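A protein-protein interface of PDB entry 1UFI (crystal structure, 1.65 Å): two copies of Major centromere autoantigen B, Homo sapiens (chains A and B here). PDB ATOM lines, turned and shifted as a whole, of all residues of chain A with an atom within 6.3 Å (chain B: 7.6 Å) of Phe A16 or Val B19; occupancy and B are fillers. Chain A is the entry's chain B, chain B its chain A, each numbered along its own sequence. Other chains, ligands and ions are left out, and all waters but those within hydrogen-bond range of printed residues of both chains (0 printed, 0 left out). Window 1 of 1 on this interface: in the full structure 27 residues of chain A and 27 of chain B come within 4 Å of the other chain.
The guanidinium group (NE) of Arg A21 is in hydrogen-bond range of the backbone carbonyl oxygen (O) of Met B4 (2.9 Å).
The side-chain sulfur (SD) of Met B18 sits close to the guanidinium group (NH2) of Arg B21 (3.8 Å). O of Tyr B22 is in hydrogen-bond range of OG of Ser B25.
CG2 of Val B19 touches O of Ala A12, 3.98 Å away. Tyr A15 touches Tyr B15 (CD2 to CD1, 3.5 Å). Tyr A15 touches Met B18 (CD1 to CB, 3.4 Å). Tyr A15 touches Val B19. Phe A16 touches Val B19. Phe A16 touches Leu B39 (CE1 to CD2, 3.9 Å). CB of Ala A17 touches CG of Met B4 (3.9 Å). O of Ala B12 touches CG2 of Val A19, at 3.5 Å. Phe B16 touches Leu A39. Leu B23 touches Leu A43 (CD2 to CD2, 3.97 Å).
Phe A16 touches just these residues of chain B: Val B19 and Leu B39. Of the printed residues of chain A, Val B19 touches Ala A12 (3.98 Å), Tyr A15 (3.8 Å), Phe A16 (3.6 Å) and Leu A43 (3.99 Å). Of the printed residues of chain A, Tyr B22 touches Pro A7 (3.3 Å), Ala A12 (3.5 Å) and Leu A43 (3.7 Å). Of the printed residues of chain B, Ala A12 touches Val B19 (3.98 Å) and Tyr B22 (3.5 Å). Printed residues of chain A within 4 Å of Ile B36: Leu A39. Of the printed residues of chain B, Ala A14 touches Met B4. Of the printed residues of chain A, Leu B23 touches Leu A39 (3.6 Å) and Leu A43 (3.97 Å). Lys B20 touches none of the printed residues of chain A. Glu A11 touches none of the printed residues of chain B. The nearest printed residue of chain A that does not touch Val B19 is Leu A39 (4.3 Å). The nearest printed residue of chain A that does not touch Met B4 is Met A13 (5.6 Å).
Of the 18 printed residues of chain A, 11 touch a printed residue of chain B. Among the printed residues, 25 pairs touch across the chains. Among the printed residues, no Asp or Glu carboxylate lies within 4 Å of a Lys or Arg side-chain nitrogen of the other chain.
Ala A12 touches Val B19, and with the chains exchanged Val A19 touches Ala B12. Tyr A15 touches Met B18, and with the chains exchanged Met A18 touches Tyr B15. Phe A16 touches Val B19, and with the chains exchanged Val A19 touches Phe B16. Leu A39 touches its own counterpart, Leu B39. Positions printed for both chains: 12, 13, 14, 15, 16, 17, 18, 19, 20, 21, 36 and 39.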
ATOM      1  N   PRO A   7      29.284 -20.627  16.438  1.00  0.00           N
ATOM      2  CA  PRO A   7      30.446 -21.403  16.027  1.00  0.00           C
ATOM      3  C   PRO A   7      30.238 -21.988  14.619  1.00  0.00           C
ATOM      4  O   PRO A   7      29.096 -22.198  14.186  1.00  0.00           O
ATOM      5  CB  PRO A   7      30.485 -22.561  17.044  1.00  0.00           C
ATOM      6  CG  PRO A   7      29.738 -22.076  18.243  1.00  0.00           C
ATOM      7  CD  PRO A   7      28.688 -21.137  17.701  1.00  0.00           C
ATOM      8  N   GLU A  11      34.223 -25.880  14.942  1.00  0.00           N
ATOM      9  CA  GLU A  11      34.279 -25.399  16.349  1.00  0.00           C
ATOM     10  C   GLU A  11      33.258 -26.153  17.202  1.00  0.00           C
ATOM     11  O   GLU A  11      33.572 -26.631  18.308  1.00  0.00           O
ATOM     12  CB  GLU A  11      34.039 -23.902  16.431  1.00  0.00           C
ATOM     13  CG  GLU A  11      35.288 -23.054  16.246  1.00  0.00           C
ATOM     14  CD  GLU A  11      34.982 -21.659  15.737  1.00  0.00           C
ATOM     15  OE1 GLU A  11      33.785 -21.261  15.654  1.00  0.00           O
ATOM     16  OE2 GLU A  11      35.967 -20.940  15.404  1.00  0.00           O
ATOM     17  N   ALA A  12      32.020 -26.272  16.707  1.00  0.00           N
ATOM     18  CA  ALA A  12      30.999 -27.048  17.438  1.00  0.00           C
ATOM     19  C   ALA A  12      31.482 -28.451  17.825  1.00  0.00           C
ATOM     20  O   ALA A  12      31.288 -28.894  18.944  1.00  0.00           O
ATOM     21  CB  ALA A  12      29.677 -27.156  16.604  1.00  0.00           C
ATOM     22  N   MET A  13      32.066 -29.155  16.855  1.00  0.00           N
ATOM     23  CA  MET A  13      32.559 -30.500  17.060  1.00  0.00           C
ATOM     24  C   MET A  13      33.739 -30.504  18.011  1.00  0.00           C
ATOM     25  O   MET A  13      33.890 -31.472  18.789  1.00  0.00           O
ATOM     26  CB  MET A  13      32.977 -31.169  15.727  1.00  0.00           C
ATOM     27  CG  MET A  13      31.758 -31.492  14.760  1.00  0.00           C
ATOM     28  SD  MET A  13      30.244 -32.177  15.592  1.00  0.00           S
ATOM     29  CE  MET A  13      30.484 -33.397  15.916  1.00  0.00           C
ATOM     30  N   ALA A  14      34.575 -29.484  17.946  1.00  0.00           N
ATOM     31  CA  ALA A  14      35.679 -29.360  18.934  1.00  0.00           C
ATOM     32  C   ALA A  14      35.189 -29.132  20.380  1.00  0.00           C
ATOM     33  O   ALA A  14      35.625 -29.807  21.307  1.00  0.00           O
ATOM     34  CB  ALA A  14      36.631 -28.269  18.525  1.00  0.00           C
ATOM     35  N   TYR A  15      34.243 -28.217  20.544  1.00  0.00           N
ATOM     36  CA  TYR A  15      33.671 -27.925  21.883  1.00  0.00           C
ATOM     37  C   TYR A  15      32.980 -29.185  22.386  1.00  0.00           C
ATOM     38  O   TYR A  15      33.154 -29.573  23.552  1.00  0.00           O
ATOM     39  CB  TYR A  15      32.628 -26.833  21.748  1.00  0.00           C
ATOM     40  CG  TYR A  15      33.160 -25.435  21.480  1.00  0.00           C
ATOM     41  CD1 TYR A  15      32.572 -24.615  20.517  1.00  0.00           C
ATOM     42  CD2 TYR A  15      34.232 -24.912  22.247  1.00  0.00           C
ATOM     43  CE1 TYR A  15      33.029 -23.312  20.315  1.00  0.00           C
ATOM     44  CE2 TYR A  15      34.671 -23.656  22.047  1.00  0.00           C
ATOM     45  CZ  TYR A  15      34.084 -22.869  21.064  1.00  0.00           C
ATOM     46  OH  TYR A  15      34.518 -21.616  20.879  1.00  0.00           O
ATOM     47  N   PHE A  16      32.214 -29.858  21.512  1.00  0.00           N
ATOM     48  CA  PHE A  16      31.569 -31.117  21.912  1.00  0.00           C
ATOM     49  C   PHE A  16      32.593 -32.186  22.315  1.00  0.00           C
ATOM     50  O   PHE A  16      32.376 -32.862  23.293  1.00  0.00           O
ATOM     51  CB  PHE A  16      30.631 -31.670  20.835  1.00  0.00           C
ATOM     52  CG  PHE A  16      29.902 -32.909  21.302  1.00  0.00           C
ATOM     53  CD1 PHE A  16      28.781 -32.794  22.126  1.00  0.00           C
ATOM     54  CD2 PHE A  16      30.400 -34.170  20.992  1.00  0.00           C
ATOM     55  CE1 PHE A  16      28.148 -34.006  22.643  1.00  0.00           C
ATOM     56  CE2 PHE A  16      29.781 -35.317  21.436  1.00  0.00           C
ATOM     57  CZ  PHE A  16      28.647 -35.213  22.274  1.00  0.00           C
ATOM     58  N   ALA A  17      33.671 -32.344  21.544  1.00  0.00           N
ATOM     59  CA  ALA A  17      34.734 -33.288  21.832  1.00  0.00           C
ATOM     60  C   ALA A  17      35.268 -33.107  23.291  1.00  0.00           C
ATOM     61  O   ALA A  17      35.436 -34.096  24.047  1.00  0.00           O
ATOM     62  CB  ALA A  17      35.850 -33.062  20.790  1.00  0.00           C
ATOM     63  N   MET A  18      35.477 -31.867  23.656  1.00  0.00           N
ATOM     64  CA  MET A  18      36.020 -31.505  24.967  1.00  0.00           C
ATOM     65  C   MET A  18      34.964 -31.725  26.051  1.00  0.00           C
ATOM     66  O   MET A  18      35.282 -32.245  27.132  1.00  0.00           O
ATOM     67  CB  MET A  18      36.547 -30.071  24.926  1.00  0.00           C
ATOM     68  CG  MET A  18      37.958 -30.008  24.128  1.00  0.00           C
ATOM     69  SD  MET A  18      38.761 -28.458  24.179  1.00  0.00           S
ATOM     70  CE  MET A  18      37.512 -27.328  23.365  1.00  0.00           C
ATOM     71  N   VAL A  19      33.700 -31.416  25.730  1.00  0.00           N
ATOM     72  CA  VAL A  19      32.585 -31.740  26.641  1.00  0.00           C
ATOM     73  C   VAL A  19      32.559 -33.242  26.888  1.00  0.00           C
ATOM     74  O   VAL A  19      32.418 -33.711  28.035  1.00  0.00           O
ATOM     75  CB  VAL A  19      31.173 -31.289  26.106  1.00  0.00           C
ATOM     76  CG1 VAL A  19      30.041 -31.959  26.967  1.00  0.00           C
ATOM     77  CG2 VAL A  19      30.998 -29.755  26.089  1.00  0.00           C
ATOM     78  N   LYS A  20      32.777 -34.020  25.826  1.00  0.00           N
ATOM     79  CA  LYS A  20      32.763 -35.520  25.932  1.00  0.00           C
ATOM     80  C   LYS A  20      33.956 -36.062  26.748  1.00  0.00           C
ATOM     81  O   LYS A  20      33.802 -36.924  27.625  1.00  0.00           O
ATOM     82  CB  LYS A  20      32.759 -36.121  24.503  1.00  0.00           C
ATOM     83  CG  LYS A  20      32.579 -37.639  24.449  1.00  0.00           C
ATOM     84  CD  LYS A  20      32.643 -38.101  22.970  1.00  0.00           C
ATOM     85  CE  LYS A  20      32.538 -39.596  22.801  1.00  0.00           C
ATOM     86  NZ  LYS A  20      32.426 -39.876  21.326  1.00  0.00           N
ATOM     87  N   ARG A  21      35.143 -35.558  26.447  1.00  0.00           N
ATOM     88  CA  ARG A  21      36.340 -35.826  27.195  1.00  0.00           C
ATOM     89  C   ARG A  21      36.125 -35.505  28.661  1.00  0.00           C
ATOM     90  O   ARG A  21      36.463 -36.308  29.511  1.00  0.00           O
ATOM     91  CB  ARG A  21      37.452 -34.934  26.645  1.00  0.00           C
ATOM     92  CG  ARG A  21      37.921 -35.444  25.288  1.00  0.00           C
ATOM     93  CD  ARG A  21      38.705 -36.750  25.345  1.00  0.00           C
ATOM     94  NE  ARG A  21      39.981 -36.579  26.028  1.00  0.00           N
ATOM     95  CZ  ARG A  21      40.746 -37.590  26.431  1.00  0.00           C
ATOM     96  NH1 ARG A  21      40.371 -38.838  26.208  1.00  0.00           N
ATOM     97  NH2 ARG A  21      41.893 -37.349  27.053  1.00  0.00           N
ATOM     98  N   HIS A  35      23.041 -40.375  26.400  1.00  0.00           N
ATOM     99  CA  HIS A  35      22.878 -38.932  26.151  1.00  0.00           C
ATOM    100  C   HIS A  35      24.013 -38.296  25.356  1.00  0.00           C
ATOM    101  O   HIS A  35      23.754 -37.443  24.478  1.00  0.00           O
ATOM    102  CB  HIS A  35      22.666 -38.237  27.474  1.00  0.00           C
ATOM    103  CG  HIS A  35      21.439 -38.673  28.197  1.00  0.00           C
ATOM    104  ND1 HIS A  35      21.270 -38.454  29.534  1.00  0.00           N
ATOM    105  CD2 HIS A  35      20.295 -39.277  27.767  1.00  0.00           C
ATOM    106  CE1 HIS A  35      20.094 -38.924  29.918  1.00  0.00           C
ATOM    107  NE2 HIS A  35      19.476 -39.406  28.854  1.00  0.00           N
ATOM    108  N   ILE A  36      25.254 -38.742  25.579  1.00  0.00           N
ATOM    109  CA  ILE A  36      26.342 -38.290  24.743  1.00  0.00           C
ATOM    110  C   ILE A  36      26.098 -38.620  23.258  1.00  0.00           C
ATOM    111  O   ILE A  36      26.167 -37.756  22.393  1.00  0.00           O
ATOM    112  CB  ILE A  36      27.653 -38.896  25.202  1.00  0.00           C
ATOM    113  CG1 ILE A  36      27.948 -38.429  26.606  1.00  0.00           C
ATOM    114  CG2 ILE A  36      28.784 -38.476  24.317  1.00  0.00           C
ATOM    115  CD1 ILE A  36      29.219 -39.079  27.205  1.00  0.00           C
ATOM    116  N   LEU A  37      25.772 -39.880  23.005  1.00  0.00           N
ATOM    117  CA  LEU A  37      25.632 -40.391  21.660  1.00  0.00           C
ATOM    118  C   LEU A  37      24.442 -39.710  20.986  1.00  0.00           C
ATOM    119  O   LEU A  37      24.540 -39.372  19.818  1.00  0.00           O
ATOM    120  CB  LEU A  37      25.424 -41.917  21.712  1.00  0.00           C
ATOM    121  CG  LEU A  37      26.659 -42.755  22.104  1.00  0.00           C
ATOM    122  CD1 LEU A  37      26.252 -44.144  22.590  1.00  0.00           C
ATOM    123  CD2 LEU A  37      27.633 -42.822  20.957  1.00  0.00           C
ATOM    124  N   LEU A  39      23.307 -36.596  21.410  1.00  0.00           N
ATOM    125  CA  LEU A  39      23.683 -35.245  20.981  1.00  0.00           C
ATOM    126  C   LEU A  39      24.770 -35.263  19.895  1.00  0.00           C
ATOM    127  O   LEU A  39      24.756 -34.396  19.010  1.00  0.00           O
ATOM    128  CB  LEU A  39      24.044 -34.318  22.208  1.00  0.00           C
ATOM    129  CG  LEU A  39      23.878 -32.806  22.033  1.00  0.00           C
ATOM    130  CD1 LEU A  39      22.421 -32.353  21.803  1.00  0.00           C
ATOM    131  CD2 LEU A  39      24.436 -32.048  23.213  1.00  0.00           C
ATOM    132  N   GLU A  40      25.715 -36.223  19.918  1.00  0.00           N
ATOM    133  CA  GLU A  40      26.741 -36.254  18.870  1.00  0.00           C
ATOM    134  C   GLU A  40      26.057 -36.508  17.497  1.00  0.00           C
ATOM    135  O   GLU A  40      26.406 -35.856  16.506  1.00  0.00           O
ATOM    136  CB  GLU A  40      27.842 -37.256  19.154  1.00  0.00           C
ATOM    137  CG  GLU A  40      29.098 -37.091  18.306  1.00  0.00           C
ATOM    138  CD  GLU A  40      30.348 -37.738  18.913  1.00  0.00           C
ATOM    139  OE1 GLU A  40      31.457 -37.471  18.363  1.00  0.00           O
ATOM    140  OE2 GLU A  40      30.251 -38.545  19.891  1.00  0.00           O
ATOM    141  N   LEU A  43      24.341 -33.331  16.365  1.00  0.00           N
ATOM    142  CA  LEU A  43      25.255 -32.339  15.790  1.00  0.00           C
ATOM    143  C   LEU A  43      25.595 -32.609  14.328  1.00  0.00           C
ATOM    144  O   LEU A  43      25.725 -31.683  13.576  1.00  0.00           O
ATOM    145  CB  LEU A  43      26.555 -32.195  16.597  1.00  0.00           C
ATOM    146  CG  LEU A  43      26.322 -31.373  17.873  1.00  0.00           C
ATOM    147  CD1 LEU A  43      27.403 -31.828  18.895  1.00  0.00           C
ATOM    148  CD2 LEU A  43      26.461 -29.914  17.638  1.00  0.00           C
ATOM    149  N   MET B   4      41.698 -35.152  22.320  1.00  0.00           N
ATOM    150  CA  MET B   4      41.350 -33.764  22.649  1.00  0.00           C
ATOM    151  C   MET B   4      41.573 -33.549  24.153  1.00  0.00           C
ATOM    152  O   MET B   4      41.659 -34.534  24.880  1.00  0.00           O
ATOM    153  CB  MET B   4      39.906 -33.442  22.203  1.00  0.00           C
ATOM    154  CG  MET B   4      39.735 -33.590  20.704  1.00  0.00           C
ATOM    155  SD  MET B   4      40.367 -32.072  19.888  1.00  0.00           S
ATOM    156  CE  MET B   4      39.191 -30.994  20.501  1.00  0.00           C
ATOM    157  N   ALA B  12      34.276 -26.864  30.555  1.00  0.00           N
ATOM    158  CA  ALA B  12      33.358 -27.787  29.858  1.00  0.00           C
ATOM    159  C   ALA B  12      31.995 -27.133  29.659  1.00  0.00           C
ATOM    160  O   ALA B  12      31.321 -27.294  28.617  1.00  0.00           O
ATOM    161  CB  ALA B  12      33.240 -29.123  30.588  1.00  0.00           C
ATOM    162  N   MET B  13      31.535 -26.414  30.682  1.00  0.00           N
ATOM    163  CA  MET B  13      30.226 -25.784  30.583  1.00  0.00           C
ATOM    164  C   MET B  13      30.221 -24.633  29.609  1.00  0.00           C
ATOM    165  O   MET B  13      29.178 -24.379  28.981  1.00  0.00           O
ATOM    166  CB  MET B  13      29.696 -25.372  31.979  1.00  0.00           C
ATOM    167  CG  MET B  13      29.604 -26.566  32.897  1.00  0.00           C
ATOM    168  SD  MET B  13      28.639 -28.049  32.205  1.00  0.00           S
ATOM    169  CE  MET B  13      27.371 -27.409  32.219  1.00  0.00           C
ATOM    170  N   ALA B  14      31.346 -23.909  29.535  1.00  0.00           N
ATOM    171  CA  ALA B  14      31.500 -22.835  28.537  1.00  0.00           C
ATOM    172  C   ALA B  14      31.372 -23.419  27.140  1.00  0.00           C
ATOM    173  O   ALA B  14      30.637 -22.905  26.296  1.00  0.00           O
ATOM    174  CB  ALA B  14      32.842 -22.098  28.713  1.00  0.00           C
ATOM    175  N   TYR B  15      32.109 -24.491  26.915  1.00  0.00           N
ATOM    176  CA  TYR B  15      32.085 -25.262  25.622  1.00  0.00           C
ATOM    177  C   TYR B  15      30.685 -25.764  25.337  1.00  0.00           C
ATOM    178  O   TYR B  15      30.189 -25.684  24.249  1.00  0.00           O
ATOM    179  CB  TYR B  15      33.020 -26.435  25.709  1.00  0.00           C
ATOM    180  CG  TYR B  15      34.484 -26.045  25.984  1.00  0.00           C
ATOM    181  CD1 TYR B  15      34.951 -24.758  25.718  1.00  0.00           C
ATOM    182  CD2 TYR B  15      35.353 -26.987  26.486  1.00  0.00           C
ATOM    183  CE1 TYR B  15      36.314 -24.417  25.991  1.00  0.00           C
ATOM    184  CE2 TYR B  15      36.684 -26.659  26.747  1.00  0.00           C
ATOM    185  CZ  TYR B  15      37.134 -25.415  26.500  1.00  0.00           C
ATOM    186  OH  TYR B  15      38.476 -25.199  26.775  1.00  0.00           O
ATOM    187  N   PHE B  16      30.031 -26.348  26.334  1.00  0.00           N
ATOM    188  CA  PHE B  16      28.662 -26.786  26.150  1.00  0.00           C
ATOM    189  C   PHE B  16      27.673 -25.677  25.750  1.00  0.00           C
ATOM    190  O   PHE B  16      26.772 -25.881  24.896  1.00  0.00           O
ATOM    191  CB  PHE B  16      28.138 -27.501  27.435  1.00  0.00           C
ATOM    192  CG  PHE B  16      26.811 -28.153  27.185  1.00  0.00           C
ATOM    193  CD1 PHE B  16      25.624 -27.536  27.511  1.00  0.00           C
ATOM    194  CD2 PHE B  16      26.801 -29.365  26.469  1.00  0.00           C
ATOM    195  CE1 PHE B  16      24.391 -28.155  27.148  1.00  0.00           C
ATOM    196  CE2 PHE B  16      25.591 -30.006  26.165  1.00  0.00           C
ATOM    197  CZ  PHE B  16      24.392 -29.360  26.476  1.00  0.00           C
ATOM    198  N   ALA B  17      27.869 -24.480  26.313  1.00  0.00           N
ATOM    199  CA  ALA B  17      27.088 -23.300  25.944  1.00  0.00           C
ATOM    200  C   ALA B  17      27.242 -23.002  24.424  1.00  0.00           C
ATOM    201  O   ALA B  17      26.268 -22.677  23.753  1.00  0.00           O
ATOM    202  CB  ALA B  17      27.499 -22.081  26.836  1.00  0.00           C
ATOM    203  N   MET B  18      28.452 -23.185  23.919  1.00  0.00           N
ATOM    204  CA  MET B  18      28.738 -22.930  22.524  1.00  0.00           C
ATOM    205  C   MET B  18      28.126 -24.058  21.664  1.00  0.00           C
ATOM    206  O   MET B  18      27.617 -23.788  20.587  1.00  0.00           O
ATOM    207  CB  MET B  18      30.271 -22.819  22.305  1.00  0.00           C
ATOM    208  CG  MET B  18      30.866 -21.575  22.957  1.00  0.00           C
ATOM    209  SD  MET B  18      30.231 -20.036  22.208  1.00  0.00           S
ATOM    210  CE  MET B  18      29.537 -19.605  23.060  1.00  0.00           C
ATOM    211  N   VAL B  19      28.198 -25.309  22.111  1.00  0.00           N
ATOM    212  CA  VAL B  19      27.468 -26.409  21.430  1.00  0.00           C
ATOM    213  C   VAL B  19      25.950 -26.077  21.337  1.00  0.00           C
ATOM    214  O   VAL B  19      25.335 -26.299  20.271  1.00  0.00           O
ATOM    215  CB  VAL B  19      27.660 -27.802  22.152  1.00  0.00           C
ATOM    216  CG1 VAL B  19      26.756 -28.870  21.497  1.00  0.00           C
ATOM    217  CG2 VAL B  19      29.122 -28.225  22.214  1.00  0.00           C
ATOM    218  N   LYS B  20      25.354 -25.589  22.430  1.00  0.00           N
ATOM    219  CA  LYS B  20      23.937 -25.236  22.442  1.00  0.00           C
ATOM    220  C   LYS B  20      23.658 -24.040  21.468  1.00  0.00           C
ATOM    221  O   LYS B  20      22.651 -24.021  20.749  1.00  0.00           O
ATOM    222  CB  LYS B  20      23.481 -24.989  23.939  1.00  0.00           C
ATOM    223  CG  LYS B  20      22.002 -24.572  24.166  1.00  0.00           C
ATOM    224  CD  LYS B  20      21.637 -24.821  25.655  1.00  0.00           C
ATOM    225  CE  LYS B  20      22.344 -23.926  26.630  1.00  0.00           C
ATOM    226  NZ  LYS B  20      21.665 -24.017  27.999  1.00  0.00           N
ATOM    227  N   ARG B  21      24.587 -23.110  21.414  1.00  0.00           N
ATOM    228  CA  ARG B  21      24.453 -21.925  20.548  1.00  0.00           C
ATOM    229  C   ARG B  21      24.444 -22.364  19.102  1.00  0.00           C
ATOM    230  O   ARG B  21      23.663 -21.834  18.267  1.00  0.00           O
ATOM    231  CB  ARG B  21      25.591 -20.935  20.811  1.00  0.00           C
ATOM    232  CG  ARG B  21      25.808 -19.980  19.648  1.00  0.00           C
ATOM    233  CD  ARG B  21      26.507 -18.711  20.037  1.00  0.00           C
ATOM    234  NE  ARG B  21      26.379 -18.482  21.459  1.00  0.00           N
ATOM    235  CZ  ARG B  21      26.871 -17.440  22.111  1.00  0.00           C
ATOM    236  NH1 ARG B  21      26.198 -16.845  23.089  1.00  0.00           N
ATOM    237  NH2 ARG B  21      28.052 -16.985  21.764  1.00  0.00           N
ATOM    238  N   TYR B  22      25.292 -23.337  18.798  1.00  0.00           N
ATOM    239  CA  TYR B  22      25.368 -23.897  17.458  1.00  0.00           C
ATOM    240  C   TYR B  22      24.075 -24.617  17.045  1.00  0.00           C
ATOM    241  O   TYR B  22      23.430 -24.301  16.004  1.00  0.00           O
ATOM    242  CB  TYR B  22      26.619 -24.796  17.279  1.00  0.00           C
ATOM    243  CG  TYR B  22      26.684 -25.469  15.938  1.00  0.00           C
ATOM    244  CD1 TYR B  22      27.162 -24.762  14.822  1.00  0.00           C
ATOM    245  CD2 TYR B  22      26.239 -26.780  15.761  1.00  0.00           C
ATOM    246  CE1 TYR B  22      27.194 -25.355  13.617  1.00  0.00           C
ATOM    247  CE2 TYR B  22      26.319 -27.404  14.518  1.00  0.00           C
ATOM    248  CZ  TYR B  22      26.759 -26.619  13.452  1.00  0.00           C
ATOM    249  OH  TYR B  22      26.804 -27.185  12.212  1.00  0.00           O
ATOM    250  N   LEU B  23      23.657 -25.537  17.869  1.00  0.00           N
ATOM    251  CA  LEU B  23      22.495 -26.354  17.600  1.00  0.00           C
ATOM    252  C   LEU B  23      21.228 -25.543  17.498  1.00  0.00           C
ATOM    253  O   LEU B  23      20.452 -25.752  16.557  1.00  0.00           O
ATOM    254  CB  LEU B  23      22.367 -27.356  18.757  1.00  0.00           C
ATOM    255  CG  LEU B  23      22.268 -28.816  18.393  1.00  0.00           C
ATOM    256  CD1 LEU B  23      22.614 -29.205  16.920  1.00  0.00           C
ATOM    257  CD2 LEU B  23      22.968 -29.654  19.508  1.00  0.00           C
ATOM    258  N   THR B  24      20.993 -24.638  18.446  1.00  0.00           N
ATOM    259  CA  THR B  24      19.768 -23.802  18.404  1.00  0.00           C
ATOM    260  C   THR B  24      19.858 -22.691  17.330  1.00  0.00           C
ATOM    261  O   THR B  24      18.953 -21.868  17.231  1.00  0.00           O
ATOM    262  CB  THR B  24      19.477 -23.145  19.790  1.00  0.00           C
ATOM    263  OG1 THR B  24      20.589 -22.325  20.144  1.00  0.00           O
ATOM    264  CG2 THR B  24      19.421 -24.188  20.850  1.00  0.00           C
ATOM    265  N   SER B  25      20.936 -22.654  16.543  1.00  0.00           N
ATOM    266  CA  SER B  25      21.024 -21.647  15.456  1.00  0.00           C
ATOM    267  C   SER B  25      20.254 -22.187  14.235  1.00  0.00           C
ATOM    268  O   SER B  25      20.021 -21.436  13.225  1.00  0.00           O
ATOM    269  CB  SER B  25      22.481 -21.341  15.080  1.00  0.00           C
ATOM    270  OG  SER B  25      23.043 -22.331  14.228  1.00  0.00           O
ATOM    271  N   ILE B  28      15.083 -26.344  15.304  1.00  0.00           N
ATOM    272  CA  ILE B  28      15.391 -27.467  16.228  1.00  0.00           C
ATOM    273  C   ILE B  28      14.114 -28.215  16.626  1.00  0.00           C
ATOM    274  O   ILE B  28      13.198 -27.563  17.026  1.00  0.00           O
ATOM    275  CB  ILE B  28      16.127 -26.831  17.512  1.00  0.00           C
ATOM    276  CG1 ILE B  28      17.131 -27.746  18.156  1.00  0.00           C
ATOM    277  CG2 ILE B  28      15.125 -26.165  18.490  1.00  0.00           C
ATOM    278  CD1 ILE B  28      17.929 -27.046  19.202  1.00  0.00           C
ATOM    279  N   ILE B  36      19.625 -31.803  24.360  1.00  0.00           N
ATOM    280  CA  ILE B  36      20.461 -30.745  24.950  1.00  0.00           C
ATOM    281  C   ILE B  36      20.271 -30.670  26.461  1.00  0.00           C
ATOM    282  O   ILE B  36      21.259 -30.686  27.207  1.00  0.00           O
ATOM    283  CB  ILE B  36      20.131 -29.383  24.329  1.00  0.00           C
ATOM    284  CG1 ILE B  36      20.648 -29.402  22.911  1.00  0.00           C
ATOM    285  CG2 ILE B  36      20.861 -28.260  25.095  1.00  0.00           C
ATOM    286  CD1 ILE B  36      20.134 -28.137  22.078  1.00  0.00           C
ATOM    287  N   LEU B  39      21.751 -33.681  28.411  1.00  0.00           N
ATOM    288  CA  LEU B  39      23.231 -33.690  28.566  1.00  0.00           C
ATOM    289  C   LEU B  39      23.730 -32.606  29.534  1.00  0.00           C
ATOM    290  O   LEU B  39      24.638 -32.848  30.328  1.00  0.00           O
ATOM    291  CB  LEU B  39      23.914 -33.662  27.181  1.00  0.00           C
ATOM    292  CG  LEU B  39      25.385 -34.029  27.339  1.00  0.00           C
ATOM    293  CD1 LEU B  39      25.530 -35.414  27.860  1.00  0.00           C
ATOM    294  CD2 LEU B  39      26.026 -33.846  25.919  1.00  0.00           C
